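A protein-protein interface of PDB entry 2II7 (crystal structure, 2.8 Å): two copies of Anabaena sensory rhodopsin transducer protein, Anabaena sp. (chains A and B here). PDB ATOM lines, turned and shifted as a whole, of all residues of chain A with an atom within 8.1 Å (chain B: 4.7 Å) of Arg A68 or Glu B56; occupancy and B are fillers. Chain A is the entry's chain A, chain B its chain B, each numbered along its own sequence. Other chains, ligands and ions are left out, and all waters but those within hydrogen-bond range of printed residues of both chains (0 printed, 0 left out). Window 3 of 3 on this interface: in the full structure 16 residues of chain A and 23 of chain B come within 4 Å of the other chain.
Printed residues of chain B within 4 Å of Leu A3: Tyr B51 (3.0 Å). Glu A42 touches none of the printed residues of chain B. Arg A68 touches just these residues of chain B: Tyr B51 (3.96 Å) and Glu B56 (2.8 Å). Of the printed residues of chain A, Tyr B52 touches Arg A69 and Thr A70. Of chain A, only Arg A68 (2.8 Å) and Arg A69 (2.3 Å) come within 4 Å of Glu B56. Pro B57 touches none of the printed residues of chain A. The nearest residue of chain B that does not touch Arg A68 is Pro B57 (4.03 Å). The nearest residue of chain A that does not touch Glu B56 is Ala A67 (5.0 Å). The nearest printed residue of chain B that does not touch Ala A39 is Pro B57 (7.0 Å).
Of the 16 printed residues of chain A, 6 touch a printed residue of chain B. Printed residues of chain A that touch a printed residue of chain B: Leu A3, Leu A37, Ala A39, Arg A68, Arg A69 and Thr A70. Of the 7 printed residues of chain B, 5 touch a printed residue of chain A. Hydrophobic or aromatic side chains of chain B within 4 Å of the printed part of chain A: Tyr B51. Among the printed residues, Asp or Glu carboxylates within 4 Å of a Lys or Arg side-chain nitrogen of the other chain: Arg A68 with Glu B56 and Arg A69 with Glu B56.
No position is printed for both chains.
OH of Tyr B51 touches CD2 of Leu A3 (3.0 Å). Leu A37 touches Tyr B51. Tyr B51 touches Ala A39 (OH to CB, 3.7 Å). Tyr B51 touches Arg A68 (CD2 to C, 3.96 Å). Arg A69 touches Tyr B52 (CD to O, 3.3 Å). NE of Arg A69 touches C of Asp B54, at 3.9 Å. Tyr B51 touches Thr A70.
OE2 of Glu B56 lies within salt-bridge range of NH1 of Arg A68. NE of Arg A69 lies within hydrogen-bond range of O of Lys B55 (2.7 Å). OE2 of Glu B56 is in salt-bridge range of NH1 of Arg A69 (3.7 Å). N of Thr A70 lies within hydrogen-bond range of O of Tyr B52, at 3.0 Å.
O of Leu A3 is in hydrogen-bond range of N of Gly A40 (3.4 Å). The backbone carbonyl oxygen of Asn A38 is in hydrogen-bond range of the backbone NH of Arg A68 (2.8 Å). The backbone carbonyl oxygen of Arg A69 sits at hydrogen-bond distance from the backbone NH of Asn A38, 2.9 Å away. The backbone carbonyl oxygen of Gly A40 sits at hydrogen-bond distance from the backbone NH of Arg A68. NE of Arg A68 is in salt-bridge range of OD1 of Asp A41, 3.2 Å away. NZ of Lys B55 lies within salt-bridge range of OD1 of Asp B54, 3.5 Å away.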
ATOM      1  N   SER A   2     -22.635   8.228  29.884  1.00  0.00           N
ATOM      2  CA  SER A   2     -21.924   9.370  29.244  1.00  0.00           C
ATOM      3  C   SER A   2     -21.327  10.264  30.325  1.00  0.00           C
ATOM      4  O   SER A   2     -21.817  11.363  30.600  1.00  0.00           O
ATOM      5  CB  SER A   2     -22.886  10.178  28.369  1.00  0.00           C
ATOM      6  OG  SER A   2     -22.194  11.191  27.654  1.00  0.00           O
ATOM      7  N   LEU A   3     -20.258   9.773  30.936  1.00  0.00           N
ATOM      8  CA  LEU A   3     -19.573  10.489  31.996  1.00  0.00           C
ATOM      9  C   LEU A   3     -18.986  11.805  31.492  1.00  0.00           C
ATOM     10  O   LEU A   3     -17.970  11.816  30.795  1.00  0.00           O
ATOM     11  CB  LEU A   3     -18.444   9.626  32.568  1.00  0.00           C
ATOM     12  CG  LEU A   3     -18.598   8.100  32.588  1.00  0.00           C
ATOM     13  CD1 LEU A   3     -18.458   7.545  31.170  1.00  0.00           C
ATOM     14  CD2 LEU A   3     -17.528   7.491  33.494  1.00  0.00           C
ATOM     15  N   LEU A  37      -7.877  11.825  31.203  1.00  0.00           N
ATOM     16  CA  LEU A  37      -8.955  10.893  30.985  1.00  0.00           C
ATOM     17  C   LEU A  37     -10.081  11.653  30.315  1.00  0.00           C
ATOM     18  O   LEU A  37     -10.326  12.823  30.623  1.00  0.00           O
ATOM     19  CB  LEU A  37      -9.429  10.300  32.309  1.00  0.00           C
ATOM     20  CG  LEU A  37     -10.789   9.599  32.209  1.00  0.00           C
ATOM     21  CD1 LEU A  37     -10.700   8.470  31.212  1.00  0.00           C
ATOM     22  CD2 LEU A  37     -11.221   9.082  33.573  1.00  0.00           C
ATOM     23  N   ASN A  38     -10.745  10.997  29.377  1.00  0.00           N
ATOM     24  CA  ASN A  38     -11.858  11.603  28.669  1.00  0.00           C
ATOM     25  C   ASN A  38     -12.921  10.537  28.672  1.00  0.00           C
ATOM     26  O   ASN A  38     -12.992   9.724  27.760  1.00  0.00           O
ATOM     27  CB  ASN A  38     -11.476  11.961  27.224  1.00  0.00           C
ATOM     28  CG  ASN A  38     -12.648  12.473  26.424  1.00  0.00           C
ATOM     29  OD1 ASN A  38     -12.525  12.773  25.233  1.00  0.00           O
ATOM     30  ND2 ASN A  38     -13.800  12.578  27.072  1.00  0.00           N
ATOM     31  N   ALA A  39     -13.743  10.531  29.705  1.00  0.00           N
ATOM     32  CA  ALA A  39     -14.773   9.527  29.788  1.00  0.00           C
ATOM     33  C   ALA A  39     -15.997   9.958  28.986  1.00  0.00           C
ATOM     34  O   ALA A  39     -17.041   9.306  29.022  1.00  0.00           O
ATOM     35  CB  ALA A  39     -15.126   9.281  31.245  1.00  0.00           C
ATOM     36  N   GLY A  40     -15.851  11.044  28.236  1.00  0.00           N
ATOM     37  CA  GLY A  40     -16.961  11.554  27.440  1.00  0.00           C
ATOM     38  C   GLY A  40     -17.148  10.891  26.088  1.00  0.00           C
ATOM     39  O   GLY A  40     -16.363  10.032  25.693  1.00  0.00           O
ATOM     40  N   ASP A  41     -18.192  11.289  25.371  1.00  0.00           N
ATOM     41  CA  ASP A  41     -18.465  10.714  24.061  1.00  0.00           C
ATOM     42  C   ASP A  41     -17.911  11.550  22.915  1.00  0.00           C
ATOM     43  O   ASP A  41     -18.039  11.176  21.747  1.00  0.00           O
ATOM     44  CB  ASP A  41     -19.973  10.512  23.874  1.00  0.00           C
ATOM     45  CG  ASP A  41     -20.548   9.512  24.860  1.00  0.00           C
ATOM     46  OD1 ASP A  41     -19.909   8.461  25.086  1.00  0.00           O
ATOM     47  OD2 ASP A  41     -21.641   9.773  25.403  1.00  0.00           O
ATOM     48  N   GLU A  42     -17.309  12.690  23.244  1.00  0.00           N
ATOM     49  CA  GLU A  42     -16.723  13.549  22.226  1.00  0.00           C
ATOM     50  C   GLU A  42     -15.218  13.662  22.420  1.00  0.00           C
ATOM     51  O   GLU A  42     -14.719  13.805  23.544  1.00  0.00           O
ATOM     52  CB  GLU A  42     -17.334  14.949  22.242  1.00  0.00           C
ATOM     53  CG  GLU A  42     -16.627  15.899  21.259  1.00  0.00           C
ATOM     54  CD  GLU A  42     -17.274  17.269  21.167  1.00  0.00           C
ATOM     55  OE1 GLU A  42     -18.516  17.360  21.318  1.00  0.00           O
ATOM     56  OE2 GLU A  42     -16.538  18.251  20.925  1.00  0.00           O
ATOM     57  N   ASP A  43     -14.499  13.586  21.307  1.00  0.00           N
ATOM     58  CA  ASP A  43     -13.053  13.674  21.328  1.00  0.00           C
ATOM     59  C   ASP A  43     -12.632  14.965  21.997  1.00  0.00           C
ATOM     60  O   ASP A  43     -13.268  16.005  21.838  1.00  0.00           O
ATOM     61  CB  ASP A  43     -12.504  13.606  19.901  1.00  0.00           C
ATOM     62  CG  ASP A  43     -12.463  12.184  19.350  1.00  0.00           C
ATOM     63  OD1 ASP A  43     -13.076  11.273  19.952  1.00  0.00           O
ATOM     64  OD2 ASP A  43     -11.815  11.979  18.304  1.00  0.00           O
ATOM     65  N   ALA A  44     -11.545  14.888  22.746  1.00  0.00           N
ATOM     66  CA  ALA A  44     -11.039  16.037  23.461  1.00  0.00           C
ATOM     67  C   ALA A  44      -9.855  16.693  22.771  1.00  0.00           C
ATOM     68  O   ALA A  44      -8.797  16.085  22.614  1.00  0.00           O
ATOM     69  CB  ALA A  44     -10.653  15.622  24.858  1.00  0.00           C
ATOM     70  N   VAL A  65      -7.405  13.684  22.771  1.00  0.00           N
ATOM     71  CA  VAL A  65      -7.698  12.539  23.608  1.00  0.00           C
ATOM     72  C   VAL A  65      -9.070  12.100  23.154  1.00  0.00           C
ATOM     73  O   VAL A  65     -10.065  12.781  23.382  1.00  0.00           O
ATOM     74  CB  VAL A  65      -7.723  12.878  25.109  1.00  0.00           C
ATOM     75  CG1 VAL A  65      -7.993  11.614  25.909  1.00  0.00           C
ATOM     76  CG2 VAL A  65      -6.385  13.471  25.538  1.00  0.00           C
ATOM     77  N   PRO A  66      -9.126  10.956  22.468  1.00  0.00           N
ATOM     78  CA  PRO A  66     -10.352  10.363  21.932  1.00  0.00           C
ATOM     79  C   PRO A  66     -11.400  10.075  22.994  1.00  0.00           C
ATOM     80  O   PRO A  66     -11.072   9.743  24.142  1.00  0.00           O
ATOM     81  CB  PRO A  66      -9.853   9.079  21.270  1.00  0.00           C
ATOM     82  CG  PRO A  66      -8.413   9.379  20.955  1.00  0.00           C
ATOM     83  CD  PRO A  66      -7.961  10.098  22.179  1.00  0.00           C
ATOM     84  N   ALA A  67     -12.660  10.193  22.595  1.00  0.00           N
ATOM     85  CA  ALA A  67     -13.774   9.919  23.491  1.00  0.00           C
ATOM     86  C   ALA A  67     -13.599   8.563  24.181  1.00  0.00           C
ATOM     87  O   ALA A  67     -13.092   7.611  23.592  1.00  0.00           O
ATOM     88  CB  ALA A  67     -15.082   9.938  22.713  1.00  0.00           C
ATOM     89  N   ARG A  68     -14.024   8.488  25.435  1.00  0.00           N
ATOM     90  CA  ARG A  68     -13.927   7.258  26.208  1.00  0.00           C
ATOM     91  C   ARG A  68     -12.534   6.648  26.158  1.00  0.00           C
ATOM     92  O   ARG A  68     -12.382   5.446  25.964  1.00  0.00           O
ATOM     93  CB  ARG A  68     -14.965   6.246  25.712  1.00  0.00           C
ATOM     94  CG  ARG A  68     -16.377   6.573  26.159  1.00  0.00           C
ATOM     95  CD  ARG A  68     -17.422   5.690  25.506  1.00  0.00           C
ATOM     96  NE  ARG A  68     -17.823   6.185  24.192  1.00  0.00           N
ATOM     97  CZ  ARG A  68     -17.127   6.005  23.075  1.00  0.00           C
ATOM     98  NH1 ARG A  68     -15.988   5.332  23.106  1.00  0.00           N
ATOM     99  NH2 ARG A  68     -17.567   6.501  21.928  1.00  0.00           N
ATOM    100  N   ARG A  69     -11.517   7.482  26.342  1.00  0.00           N
ATOM    101  CA  ARG A  69     -10.139   7.014  26.326  1.00  0.00           C
ATOM    102  C   ARG A  69      -9.290   7.806  27.310  1.00  0.00           C
ATOM    103  O   ARG A  69      -9.679   8.881  27.748  1.00  0.00           O
ATOM    104  CB  ARG A  69      -9.552   7.164  24.923  1.00  0.00           C
ATOM    105  CG  ARG A  69     -10.204   6.278  23.883  1.00  0.00           C
ATOM    106  CD  ARG A  69      -9.579   4.896  23.860  1.00  0.00           C
ATOM    107  NE  ARG A  69     -10.570   3.839  23.669  1.00  0.00           N
ATOM    108  CZ  ARG A  69     -11.477   3.805  22.696  1.00  0.00           C
ATOM    109  NH1 ARG A  69     -11.547   4.771  21.798  1.00  0.00           N
ATOM    110  NH2 ARG A  69     -12.318   2.787  22.627  1.00  0.00           N
ATOM    111  N   THR A  70      -8.134   7.259  27.663  1.00  0.00           N
ATOM    112  CA  THR A  70      -7.203   7.921  28.566  1.00  0.00           C
ATOM    113  C   THR A  70      -5.954   8.183  27.748  1.00  0.00           C
ATOM    114  O   THR A  70      -5.850   7.726  26.609  1.00  0.00           O
ATOM    115  CB  THR A  70      -6.813   7.030  29.752  1.00  0.00           C
ATOM    116  OG1 THR A  70      -5.851   7.711  30.563  1.00  0.00           O
ATOM    117  CG2 THR A  70      -6.195   5.754  29.272  1.00  0.00           C
ATOM    118  N   TYR B  51     -10.225   2.539  31.925  1.00  0.00           N
ATOM    119  CA  TYR B  51     -10.137   3.122  30.597  1.00  0.00           C
ATOM    120  C   TYR B  51      -8.723   2.938  30.057  1.00  0.00           C
ATOM    121  O   TYR B  51      -7.753   2.915  30.814  1.00  0.00           O
ATOM    122  CB  TYR B  51     -10.482   4.616  30.641  1.00  0.00           C
ATOM    123  CG  TYR B  51     -11.942   4.935  30.924  1.00  0.00           C
ATOM    124  CD1 TYR B  51     -12.484   4.777  32.204  1.00  0.00           C
ATOM    125  CD2 TYR B  51     -12.783   5.388  29.907  1.00  0.00           C
ATOM    126  CE1 TYR B  51     -13.825   5.062  32.462  1.00  0.00           C
ATOM    127  CE2 TYR B  51     -14.129   5.672  30.156  1.00  0.00           C
ATOM    128  CZ  TYR B  51     -14.641   5.504  31.434  1.00  0.00           C
ATOM    129  OH  TYR B  51     -15.976   5.751  31.671  1.00  0.00           O
ATOM    130  N   TYR B  52      -8.609   2.802  28.742  1.00  0.00           N
ATOM    131  CA  TYR B  52      -7.304   2.613  28.112  1.00  0.00           C
ATOM    132  C   TYR B  52      -7.085   3.676  27.056  1.00  0.00           C
ATOM    133  O   TYR B  52      -7.996   4.448  26.733  1.00  0.00           O
ATOM    134  CB  TYR B  52      -7.210   1.213  27.486  1.00  0.00           C
ATOM    135  CG  TYR B  52      -7.273   0.090  28.507  1.00  0.00           C
ATOM    136  CD1 TYR B  52      -6.145  -0.263  29.254  1.00  0.00           C
ATOM    137  CD2 TYR B  52      -8.473  -0.575  28.777  1.00  0.00           C
ATOM    138  CE1 TYR B  52      -6.212  -1.239  30.246  1.00  0.00           C
ATOM    139  CE2 TYR B  52      -8.548  -1.550  29.766  1.00  0.00           C
ATOM    140  CZ  TYR B  52      -7.418  -1.877  30.503  1.00  0.00           C
ATOM    141  OH  TYR B  52      -7.507  -2.799  31.536  1.00  0.00           O
ATOM    142  N   ASP B  54      -6.100   2.991  23.844  1.00  0.00           N
ATOM    143  CA  ASP B  54      -6.374   2.499  22.496  1.00  0.00           C
ATOM    144  C   ASP B  54      -7.642   1.669  22.356  1.00  0.00           C
ATOM    145  O   ASP B  54      -8.233   1.605  21.281  1.00  0.00           O
ATOM    146  CB  ASP B  54      -5.190   1.682  22.005  1.00  0.00           C
ATOM    147  CG  ASP B  54      -4.662   0.754  23.069  1.00  0.00           C
ATOM    148  OD1 ASP B  54      -5.481   0.032  23.674  1.00  0.00           O
ATOM    149  OD2 ASP B  54      -3.435   0.750  23.302  1.00  0.00           O
ATOM    150  N   LYS B  55      -8.064   1.030  23.433  1.00  0.00           N
ATOM    151  CA  LYS B  55      -9.267   0.217  23.373  1.00  0.00           C
ATOM    152  C   LYS B  55     -10.389   0.744  24.273  1.00  0.00           C
ATOM    153  O   LYS B  55     -10.170   1.607  25.126  1.00  0.00           O
ATOM    154  CB  LYS B  55      -8.921  -1.241  23.717  1.00  0.00           C
ATOM    155  CG  LYS B  55      -7.970  -1.432  24.898  1.00  0.00           C
ATOM    156  CD  LYS B  55      -7.646  -2.915  25.103  1.00  0.00           C
ATOM    157  CE  LYS B  55      -6.661  -3.152  26.250  1.00  0.00           C
ATOM    158  NZ  LYS B  55      -5.308  -2.567  26.000  1.00  0.00           N
ATOM    159  N   GLU B  56     -11.594   0.225  24.067  1.00  0.00           N
ATOM    160  CA  GLU B  56     -12.759   0.627  24.850  1.00  0.00           C
ATOM    161  C   GLU B  56     -12.652   0.274  26.342  1.00  0.00           C
ATOM    162  O   GLU B  56     -11.854  -0.578  26.737  1.00  0.00           O
ATOM    163  CB  GLU B  56     -14.006  -0.016  24.252  1.00  0.00           C
ATOM    164  CG  GLU B  56     -14.447   0.619  22.956  1.00  0.00           C
ATOM    165  CD  GLU B  56     -15.117   1.955  23.178  1.00  0.00           C
ATOM    166  OE1 GLU B  56     -16.110   1.989  23.934  1.00  0.00           O
ATOM    167  OE2 GLU B  56     -14.660   2.965  22.598  1.00  0.00           O
ATOM    168  N   PRO B  57     -13.466   0.932  27.188  1.00  0.00           N
ATOM    169  CA  PRO B  57     -13.487   0.713  28.641  1.00  0.00           C
ATOM    170  C   PRO B  57     -13.862  -0.716  28.997  1.00  0.00           C
ATOM    171  O   PRO B  57     -14.711  -1.319  28.345  1.00  0.00           O
ATOM    172  CB  PRO B  57     -14.544   1.702  29.129  1.00  0.00           C
ATOM    173  CG  PRO B  57     -14.520   2.777  28.088  1.00  0.00           C
ATOM    174  CD  PRO B  57     -14.416   1.993  26.813  1.00  0.00           C
ATOM    175  N   VAL B  58     -13.241  -1.254  30.038  1.00  0.00           N
ATOM    176  CA  VAL B  58     -13.539  -2.615  30.457  1.00  0.00           C
ATOM    177  C   VAL B  58     -14.618  -2.568  31.524  1.00  0.00           C
ATOM    178  O   VAL B  58     -14.414  -1.974  32.572  1.00  0.00           O
ATOM    179  CB  VAL B  58     -12.281  -3.340  31.029  1.00  0.00           C
ATOM    180  CG1 VAL B  58     -12.682  -4.692  31.602  1.00  0.00           C
ATOM    181  CG2 VAL B  58     -11.224  -3.524  29.929  1.00  0.00           C
